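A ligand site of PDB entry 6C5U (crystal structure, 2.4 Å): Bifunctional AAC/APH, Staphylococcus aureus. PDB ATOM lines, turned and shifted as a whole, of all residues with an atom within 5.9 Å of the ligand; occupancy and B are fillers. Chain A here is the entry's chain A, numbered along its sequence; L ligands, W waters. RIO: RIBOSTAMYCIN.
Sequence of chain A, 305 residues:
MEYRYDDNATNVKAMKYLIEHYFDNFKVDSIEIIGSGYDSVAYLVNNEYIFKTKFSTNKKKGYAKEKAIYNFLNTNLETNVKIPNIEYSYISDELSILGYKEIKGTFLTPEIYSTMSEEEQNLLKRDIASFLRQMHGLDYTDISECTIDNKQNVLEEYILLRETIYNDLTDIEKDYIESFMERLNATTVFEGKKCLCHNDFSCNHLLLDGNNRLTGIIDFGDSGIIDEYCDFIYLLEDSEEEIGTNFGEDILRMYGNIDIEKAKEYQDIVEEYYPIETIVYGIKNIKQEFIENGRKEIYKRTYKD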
ATOM      1  N   ASP A 200       7.066 -10.189  23.632  1.00  0.00           N
ATOM      2  CA  ASP A 200       6.935 -10.188  22.154  1.00  0.00           C
ATOM      3  C   ASP A 200       7.682 -11.395  21.600  1.00  0.00           C
ATOM      4  O   ASP A 200       8.528 -11.292  20.721  1.00  0.00           O
ATOM      5  CB  ASP A 200       7.525  -8.871  21.642  1.00  0.00           C
ATOM      6  CG  ASP A 200       7.123  -8.507  20.272  1.00  0.00           C
ATOM      7  OD1 ASP A 200       6.283  -9.197  19.665  1.00  0.00           O
ATOM      8  OD2 ASP A 200       7.699  -7.487  19.814  1.00  0.00           O
ATOM      9  N   PHE A 201       7.361 -12.550  22.147  1.00  0.00           N
ATOM     10  CA  PHE A 201       8.187 -13.760  22.057  1.00  0.00           C
ATOM     11  C   PHE A 201       7.806 -14.586  20.849  1.00  0.00           C
ATOM     12  O   PHE A 201       7.171 -15.597  20.946  1.00  0.00           O
ATOM     13  CB  PHE A 201       7.988 -14.579  23.348  1.00  0.00           C
ATOM     14  CG  PHE A 201       9.067 -15.575  23.589  1.00  0.00           C
ATOM     15  CD1 PHE A 201      10.271 -15.147  24.099  1.00  0.00           C
ATOM     16  CD2 PHE A 201       8.898 -16.898  23.288  1.00  0.00           C
ATOM     17  CE1 PHE A 201      11.308 -16.022  24.285  1.00  0.00           C
ATOM     18  CE2 PHE A 201       9.920 -17.786  23.498  1.00  0.00           C
ATOM     19  CZ  PHE A 201      11.115 -17.357  24.003  1.00  0.00           C
ATOM     20  N   SER A 202       8.162 -14.095  19.693  1.00  0.00           N
ATOM     21  CA  SER A 202       7.792 -14.667  18.414  1.00  0.00           C
ATOM     22  C   SER A 202       9.030 -15.216  17.813  1.00  0.00           C
ATOM     23  O   SER A 202      10.127 -14.881  18.277  1.00  0.00           O
ATOM     24  CB  SER A 202       7.249 -13.583  17.544  1.00  0.00           C
ATOM     25  OG  SER A 202       8.025 -12.403  17.652  1.00  0.00           O
ATOM     26  N   ASN A 204      10.697 -14.659  15.061  1.00  0.00           N
ATOM     27  CA  ASN A 204      11.646 -13.647  14.533  1.00  0.00           C
ATOM     28  C   ASN A 204      12.532 -12.943  15.618  1.00  0.00           C
ATOM     29  O   ASN A 204      13.337 -12.064  15.290  1.00  0.00           O
ATOM     30  CB  ASN A 204      10.904 -12.609  13.676  1.00  0.00           C
ATOM     31  CG  ASN A 204      10.183 -11.579  14.494  1.00  0.00           C
ATOM     32  OD1 ASN A 204       9.578 -11.894  15.497  1.00  0.00           O
ATOM     33  ND2 ASN A 204      10.276 -10.361  14.111  1.00  0.00           N
ATOM     34  N   HIS A 205      12.372 -13.290  16.889  1.00  0.00           N
ATOM     35  CA  HIS A 205      13.296 -12.857  17.925  1.00  0.00           C
ATOM     36  C   HIS A 205      14.112 -13.993  18.542  1.00  0.00           C
ATOM     37  O   HIS A 205      14.837 -13.755  19.521  1.00  0.00           O
ATOM     38  CB  HIS A 205      12.545 -12.143  19.029  1.00  0.00           C
ATOM     39  CG  HIS A 205      11.875 -10.895  18.589  1.00  0.00           C
ATOM     40  ND1 HIS A 205      10.700 -10.463  19.135  1.00  0.00           N
ATOM     41  CD2 HIS A 205      12.216  -9.969  17.665  1.00  0.00           C
ATOM     42  CE1 HIS A 205      10.340  -9.311  18.584  1.00  0.00           C
ATOM     43  NE2 HIS A 205      11.241  -8.992  17.672  1.00  0.00           N
ATOM     44  N   ASP A 222       9.325  -4.748  24.808  1.00  0.00           N
ATOM     45  CA  ASP A 222       8.013  -4.655  25.374  1.00  0.00           C
ATOM     46  C   ASP A 222       7.928  -5.381  26.699  1.00  0.00           C
ATOM     47  O   ASP A 222       6.836  -5.556  27.229  1.00  0.00           O
ATOM     48  CB  ASP A 222       6.999  -5.238  24.373  1.00  0.00           C
ATOM     49  CG  ASP A 222       6.788  -4.352  23.141  1.00  0.00           C
ATOM     50  OD1 ASP A 222       7.069  -3.115  23.140  1.00  0.00           O
ATOM     51  OD2 ASP A 222       6.280  -4.943  22.178  1.00  0.00           O
ATOM     52  N   TYR A 234       2.537 -16.007  20.860  1.00  0.00           N
ATOM     53  CA  TYR A 234       3.013 -16.239  19.483  1.00  0.00           C
ATOM     54  C   TYR A 234       3.418 -17.688  19.251  1.00  0.00           C
ATOM     55  O   TYR A 234       3.217 -18.240  18.177  1.00  0.00           O
ATOM     56  CB  TYR A 234       4.102 -15.228  19.051  1.00  0.00           C
ATOM     57  CG  TYR A 234       3.635 -13.805  19.229  1.00  0.00           C
ATOM     58  CD1 TYR A 234       2.621 -13.317  18.458  1.00  0.00           C
ATOM     59  CD2 TYR A 234       4.133 -13.001  20.228  1.00  0.00           C
ATOM     60  CE1 TYR A 234       2.123 -12.005  18.638  1.00  0.00           C
ATOM     61  CE2 TYR A 234       3.666 -11.719  20.411  1.00  0.00           C
ATOM     62  CZ  TYR A 234       2.654 -11.224  19.599  1.00  0.00           C
ATOM     63  OH  TYR A 234       2.191  -9.950  19.794  1.00  0.00           O
ATOM     64  N   GLU A 237       0.382 -19.287  18.039  1.00  0.00           N
ATOM     65  CA  GLU A 237      -0.318 -18.649  16.907  1.00  0.00           C
ATOM     66  C   GLU A 237      -0.296 -19.506  15.674  1.00  0.00           C
ATOM     67  O   GLU A 237       0.720 -20.147  15.346  1.00  0.00           O
ATOM     68  CB  GLU A 237       0.386 -17.332  16.573  1.00  0.00           C
ATOM     69  CG  GLU A 237      -0.241 -16.485  15.495  1.00  0.00           C
ATOM     70  CD  GLU A 237       0.485 -15.183  15.258  1.00  0.00           C
ATOM     71  OE1 GLU A 237       0.192 -14.185  15.952  1.00  0.00           O
ATOM     72  OE2 GLU A 237       1.324 -15.108  14.310  1.00  0.00           O
ATOM     73  N   ASP A 238      -1.428 -19.514  14.991  1.00  0.00           N
ATOM     74  CA  ASP A 238      -1.559 -20.241  13.751  1.00  0.00           C
ATOM     75  C   ASP A 238      -1.485 -19.166  12.646  1.00  0.00           C
ATOM     76  O   ASP A 238      -2.421 -18.383  12.477  1.00  0.00           O
ATOM     77  CB  ASP A 238      -2.902 -21.006  13.758  1.00  0.00           C
ATOM     78  CG  ASP A 238      -3.169 -21.782  12.468  1.00  0.00           C
ATOM     79  OD1 ASP A 238      -2.200 -22.301  11.865  1.00  0.00           O
ATOM     80  OD2 ASP A 238      -4.358 -21.891  12.095  1.00  0.00           O
ATOM     81  N   SER A 239      -0.344 -19.094  11.952  1.00  0.00           N
ATOM     82  CA  SER A 239      -0.069 -18.081  10.916  1.00  0.00           C
ATOM     83  C   SER A 239       1.179 -18.454  10.105  1.00  0.00           C
ATOM     84  O   SER A 239       1.977 -19.264  10.531  1.00  0.00           O
ATOM     85  CB  SER A 239       0.152 -16.695  11.537  1.00  0.00           C
ATOM     86  OG  SER A 239       1.420 -16.596  12.200  1.00  0.00           O
ATOM     87  N   GLU A 241       3.816 -16.555   9.746  1.00  0.00           N
ATOM     88  CA  GLU A 241       5.021 -16.091  10.446  1.00  0.00           C
ATOM     89  C   GLU A 241       5.500 -17.014  11.586  1.00  0.00           C
ATOM     90  O   GLU A 241       6.680 -16.996  11.983  1.00  0.00           O
ATOM     91  CB  GLU A 241       4.798 -14.695  11.026  1.00  0.00           C
ATOM     92  CG  GLU A 241       4.754 -13.585   9.981  1.00  0.00           C
ATOM     93  CD  GLU A 241       4.257 -12.229  10.542  1.00  0.00           C
ATOM     94  OE1 GLU A 241       4.393 -11.891  11.760  1.00  0.00           O
ATOM     95  OE2 GLU A 241       3.723 -11.457   9.707  1.00  0.00           O
ATOM     96  N   GLU A 242       4.553 -17.757  12.154  1.00  0.00           N
ATOM     97  CA  GLU A 242       4.863 -18.591  13.327  1.00  0.00           C
ATOM     98  C   GLU A 242       4.771 -20.075  12.981  1.00  0.00           C
ATOM     99  O   GLU A 242       4.235 -20.459  11.950  1.00  0.00           O
ATOM    100  CB  GLU A 242       3.960 -18.243  14.510  1.00  0.00           C
ATOM    101  CG  GLU A 242       4.002 -16.791  14.952  1.00  0.00           C
ATOM    102  CD  GLU A 242       5.383 -16.275  15.335  1.00  0.00           C
ATOM    103  OE1 GLU A 242       6.147 -17.004  15.995  1.00  0.00           O
ATOM    104  OE2 GLU A 242       5.695 -15.112  14.974  1.00  0.00           O
ATOM    105  N   VAL A 270      -6.357 -11.869  22.616  1.00  0.00           N
ATOM    106  CA  VAL A 270      -5.398 -10.929  22.047  1.00  0.00           C
ATOM    107  C   VAL A 270      -5.499 -10.944  20.555  1.00  0.00           C
ATOM    108  O   VAL A 270      -5.405  -9.897  19.947  1.00  0.00           O
ATOM    109  CB  VAL A 270      -3.996 -11.264  22.511  1.00  0.00           C
ATOM    110  CG1 VAL A 270      -2.937 -10.607  21.659  1.00  0.00           C
ATOM    111  CG2 VAL A 270      -3.854 -10.862  23.989  1.00  0.00           C
ATOM    112  N   GLU A 271      -5.702 -12.096  19.944  1.00  0.00           N
ATOM    113  CA  GLU A 271      -5.852 -12.165  18.490  1.00  0.00           C
ATOM    114  C   GLU A 271      -7.139 -11.404  18.088  1.00  0.00           C
ATOM    115  O   GLU A 271      -7.135 -10.679  17.121  1.00  0.00           O
ATOM    116  CB  GLU A 271      -5.836 -13.599  17.975  1.00  0.00           C
ATOM    117  CG  GLU A 271      -5.971 -13.753  16.451  1.00  0.00           C
ATOM    118  CD  GLU A 271      -4.765 -13.239  15.653  1.00  0.00           C
ATOM    119  OE1 GLU A 271      -4.723 -12.096  15.118  1.00  0.00           O
ATOM    120  OE2 GLU A 271      -3.802 -14.032  15.549  1.00  0.00           O
ATOM    121  N   TYR A 274      -6.498  -7.611  17.907  1.00  0.00           N
ATOM    122  CA  TYR A 274      -5.519  -7.070  16.984  1.00  0.00           C
ATOM    123  C   TYR A 274      -6.038  -5.960  16.078  1.00  0.00           C
ATOM    124  O   TYR A 274      -5.407  -4.956  15.987  1.00  0.00           O
ATOM    125  CB  TYR A 274      -4.894  -8.207  16.160  1.00  0.00           C
ATOM    126  CG  TYR A 274      -3.944  -7.772  15.067  1.00  0.00           C
ATOM    127  CD1 TYR A 274      -2.743  -7.146  15.351  1.00  0.00           C
ATOM    128  CD2 TYR A 274      -4.260  -8.036  13.709  1.00  0.00           C
ATOM    129  CE1 TYR A 274      -1.867  -6.791  14.331  1.00  0.00           C
ATOM    130  CE2 TYR A 274      -3.385  -7.694  12.690  1.00  0.00           C
ATOM    131  CZ  TYR A 274      -2.206  -7.053  12.993  1.00  0.00           C
ATOM    132  OH  TYR A 274      -1.350  -6.739  11.945  1.00  0.00           O
ATOM    133  N   GLU A 277      -6.447  -2.902  18.189  1.00  0.00           N
ATOM    134  CA  GLU A 277      -5.115  -2.433  18.552  1.00  0.00           C
ATOM    135  C   GLU A 277      -4.532  -1.622  17.400  1.00  0.00           C
ATOM    136  O   GLU A 277      -3.893  -0.610  17.620  1.00  0.00           O
ATOM    137  CB  GLU A 277      -4.192  -3.611  18.896  1.00  0.00           C
ATOM    138  CG  GLU A 277      -2.800  -3.237  19.325  1.00  0.00           C
ATOM    139  CD  GLU A 277      -1.836  -4.440  19.354  1.00  0.00           C
ATOM    140  OE1 GLU A 277      -1.437  -4.950  18.324  1.00  0.00           O
ATOM    141  OE2 GLU A 277      -1.375  -4.881  20.414  1.00  0.00           O
ATOM    142  N   THR A 278      -4.788  -2.065  16.178  1.00  0.00           N
ATOM    143  CA  THR A 278      -4.311  -1.425  14.991  1.00  0.00           C
ATOM    144  C   THR A 278      -4.988  -0.048  14.858  1.00  0.00           C
ATOM    145  O   THR A 278      -4.304   0.960  14.625  1.00  0.00           O
ATOM    146  CB  THR A 278      -4.485  -2.334  13.748  1.00  0.00           C
ATOM    147  OG1 THR A 278      -3.757  -3.573  13.906  1.00  0.00           O
ATOM    148  CG2 THR A 278      -3.933  -1.642  12.539  1.00  0.00           C
ATOM    149  N   TYR A 281      -3.615   2.391  17.554  1.00  0.00           N
ATOM    150  CA  TYR A 281      -2.294   2.851  17.155  1.00  0.00           C
ATOM    151  C   TYR A 281      -2.424   3.994  16.138  1.00  0.00           C
ATOM    152  O   TYR A 281      -1.703   4.937  16.238  1.00  0.00           O
ATOM    153  CB  TYR A 281      -1.484   1.703  16.545  1.00  0.00           C
ATOM    154  CG  TYR A 281      -0.112   2.110  16.154  1.00  0.00           C
ATOM    155  CD1 TYR A 281       0.914   2.076  17.081  1.00  0.00           C
ATOM    156  CD2 TYR A 281       0.183   2.562  14.846  1.00  0.00           C
ATOM    157  CE1 TYR A 281       2.199   2.488  16.736  1.00  0.00           C
ATOM    158  CE2 TYR A 281       1.465   2.982  14.507  1.00  0.00           C
ATOM    159  CZ  TYR A 281       2.458   2.921  15.464  1.00  0.00           C
ATOM    160  OH  TYR A 281       3.702   3.307  15.145  1.00  0.00           O
ATOM    161  N   PHE A 290      -3.524   3.179   9.387  1.00  0.00           N
ATOM    162  CA  PHE A 290      -3.714   2.167  10.400  1.00  0.00           C
ATOM    163  C   PHE A 290      -5.171   2.077  10.842  1.00  0.00           C
ATOM    164  O   PHE A 290      -5.684   0.982  11.076  1.00  0.00           O
ATOM    165  CB  PHE A 290      -2.777   2.437  11.591  1.00  0.00           C
ATOM    166  CG  PHE A 290      -1.372   2.071  11.326  1.00  0.00           C
ATOM    167  CD1 PHE A 290      -0.950   0.757  11.458  1.00  0.00           C
ATOM    168  CD2 PHE A 290      -0.463   3.029  10.877  1.00  0.00           C
ATOM    169  CE1 PHE A 290       0.384   0.424  11.214  1.00  0.00           C
ATOM    170  CE2 PHE A 290       0.861   2.695  10.611  1.00  0.00           C
ATOM    171  CZ  PHE A 290       1.281   1.389  10.748  1.00  0.00           C
ATOM    172  N   ARG A 301     -12.487 -10.502   9.032  1.00  0.00           N
ATOM    173  CA  ARG A 301     -12.808 -11.471  10.071  1.00  0.00           C
ATOM    174  C   ARG A 301     -14.297 -11.737  10.226  1.00  0.00           C
ATOM    175  O   ARG A 301     -14.682 -12.869  10.441  1.00  0.00           O
ATOM    176  CB  ARG A 301     -12.245 -10.995  11.389  1.00  0.00           C
ATOM    177  CG  ARG A 301     -10.758 -11.236  11.536  1.00  0.00           C
ATOM    178  CD  ARG A 301     -10.166 -10.275  12.528  1.00  0.00           C
ATOM    179  NE  ARG A 301      -9.246 -10.813  13.560  1.00  0.00           N
ATOM    180  CZ  ARG A 301      -7.931 -10.720  13.520  1.00  0.00           C
ATOM    181  NH1 ARG A 301      -7.305 -10.201  12.480  1.00  0.00           N
ATOM    182  NH2 ARG A 301      -7.221 -11.174  14.518  1.00  0.00           N
HETATM  183  O1  RIO L   1       1.688  -2.878  15.464  1.00  0.00           O
HETATM  184  C1  RIO L   1       1.547  -3.746  14.322  1.00  0.00           C
HETATM  185  C2  RIO L   1       2.415  -5.007  14.369  1.00  0.00           C
HETATM  186  O2  RIO L   1       2.056  -5.860  15.479  1.00  0.00           O
HETATM  187  C3  RIO L   1       2.780  -7.065  15.210  1.00  0.00           C
HETATM  188  O3  RIO L   1       2.176  -8.196  15.855  1.00  0.00           O
HETATM  189  C4  RIO L   1       2.897  -9.426  16.101  1.00  0.00           C
HETATM  190  C5  RIO L   1       4.308  -9.124  16.645  1.00  0.00           C
HETATM  191  O4  RIO L   1       4.259  -8.372  17.873  1.00  0.00           O
HETATM  192  C6  RIO L   1       5.132 -10.425  16.815  1.00  0.00           C
HETATM  193  N1  RIO L   1       6.501 -10.141  17.292  1.00  0.00           N
HETATM  194  C7  RIO L   1       5.136 -11.224  15.503  1.00  0.00           C
HETATM  195  C8  RIO L   1       3.701 -11.680  15.250  1.00  0.00           C
HETATM  196  N2  RIO L   1       3.598 -12.832  14.343  1.00  0.00           N
HETATM  197  C9  RIO L   1       2.870 -10.429  14.935  1.00  0.00           C
HETATM  198  O5  RIO L   1       1.541 -10.975  14.768  1.00  0.00           O
HETATM  199  C10 RIO L   1       0.458 -10.163  14.365  1.00  0.00           C
HETATM  200  O6  RIO L   1       0.500  -9.867  12.974  1.00  0.00           O
HETATM  201  C11 RIO L   1       0.372 -10.997  12.092  1.00  0.00           C
HETATM  202  C12 RIO L   1       0.477 -10.464  10.680  1.00  0.00           C
HETATM  203  N3  RIO L   1       1.825  -9.920  10.493  1.00  0.00           N
HETATM  204  C13 RIO L   1      -0.945 -11.719  12.347  1.00  0.00           C
HETATM  205  O7  RIO L   1      -0.980 -12.911  11.575  1.00  0.00           O
HETATM  206  C14 RIO L   1      -1.055 -12.061  13.823  1.00  0.00           C
HETATM  207  O8  RIO L   1      -2.314 -12.666  14.051  1.00  0.00           O
HETATM  208  C15 RIO L   1      -0.896 -10.805  14.686  1.00  0.00           C
HETATM  209  N4  RIO L   1      -1.114 -10.949  16.145  1.00  0.00           N
HETATM  210  C16 RIO L   1       2.658  -7.291  13.696  1.00  0.00           C
HETATM  211  O9  RIO L   1       3.882  -7.846  13.211  1.00  0.00           O
HETATM  212  C17 RIO L   1       2.278  -5.911  13.140  1.00  0.00           C
HETATM  213  O10 RIO L   1       3.136  -5.477  12.080  1.00  0.00           O
HETATM  214  O   HOH W   1       3.681  -7.952  20.402  1.00  0.00           O
HETATM  215  O   HOH W   2       8.028  -8.339  15.751  1.00  0.00           O
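Residues that only touch the ligand: Tyr 274 (3.8 Å), Ser 239 (3.9 Å) and Asn 204 (3.97 Å).
A nitrogen (N4) of the ligand is in salt-bridge range of the side-chain carboxylate (OE1) of Glu 271 (3.9 Å).
N1 of the ligand is in salt-bridge range of OD1 of Asp 200 (2.6 Å).
A nitrogen (N3) of the ligand is in salt-bridge range of the side-chain carboxylate (OE2) of Glu 241 (2.6 Å).
N1 of the ligand lies within hydrogen-bond range of OG of Ser 202 (2.8 Å).
OE2 of Glu 242 lies within salt-bridge range of N2 of the ligand (3.2 Å).
The side-chain carboxylate (OE2) of Glu 237 is in salt-bridge range of a nitrogen (N2) of the ligand, 3.2 Å away.
OH of Tyr 234 sits at hydrogen-bond distance from O4 of the ligand (3.2 Å).
The side-chain carboxylate (OE1) of Glu 271 is in salt-bridge range of the guanidinium group (NH2) of Arg 301.
The backbone carbonyl oxygen (O) of Asp 200 is in hydrogen-bond range of the side-chain hydroxyl (OG) of Ser 202 (3.3 Å).
O of Asp 200 is in hydrogen-bond range of ND1 of His 205, 2.8 Å away.
The side-chain hydroxyl (OG) of Ser 239 sits close to the backbone NH (N) of Glu 241, 3.4 Å away.
The side-chain amide oxygen of Asn 204 is in hydrogen-bond range of the side-chain hydroxyl of Ser 202.
The side-chain hydroxyl (OG) of Ser 239 sits at hydrogen-bond distance from the backbone NH (N) of Glu 242 (3.3 Å).
OE2 of Glu 237 is in hydrogen-bond range of OG of Ser 239, 2.6 Å away.
O of Tyr 274 lies within hydrogen-bond range of OG1 of Thr 278 (3.0 Å).
Water W1 lies within hydrogen-bond range of OH of Tyr 234, O4 of the ligand and OD1 of Asp 200.
Water W2 lies within hydrogen-bond range of N1 of the ligand (2.8 Å) and ND2 of Asn 204 (3.4 Å).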
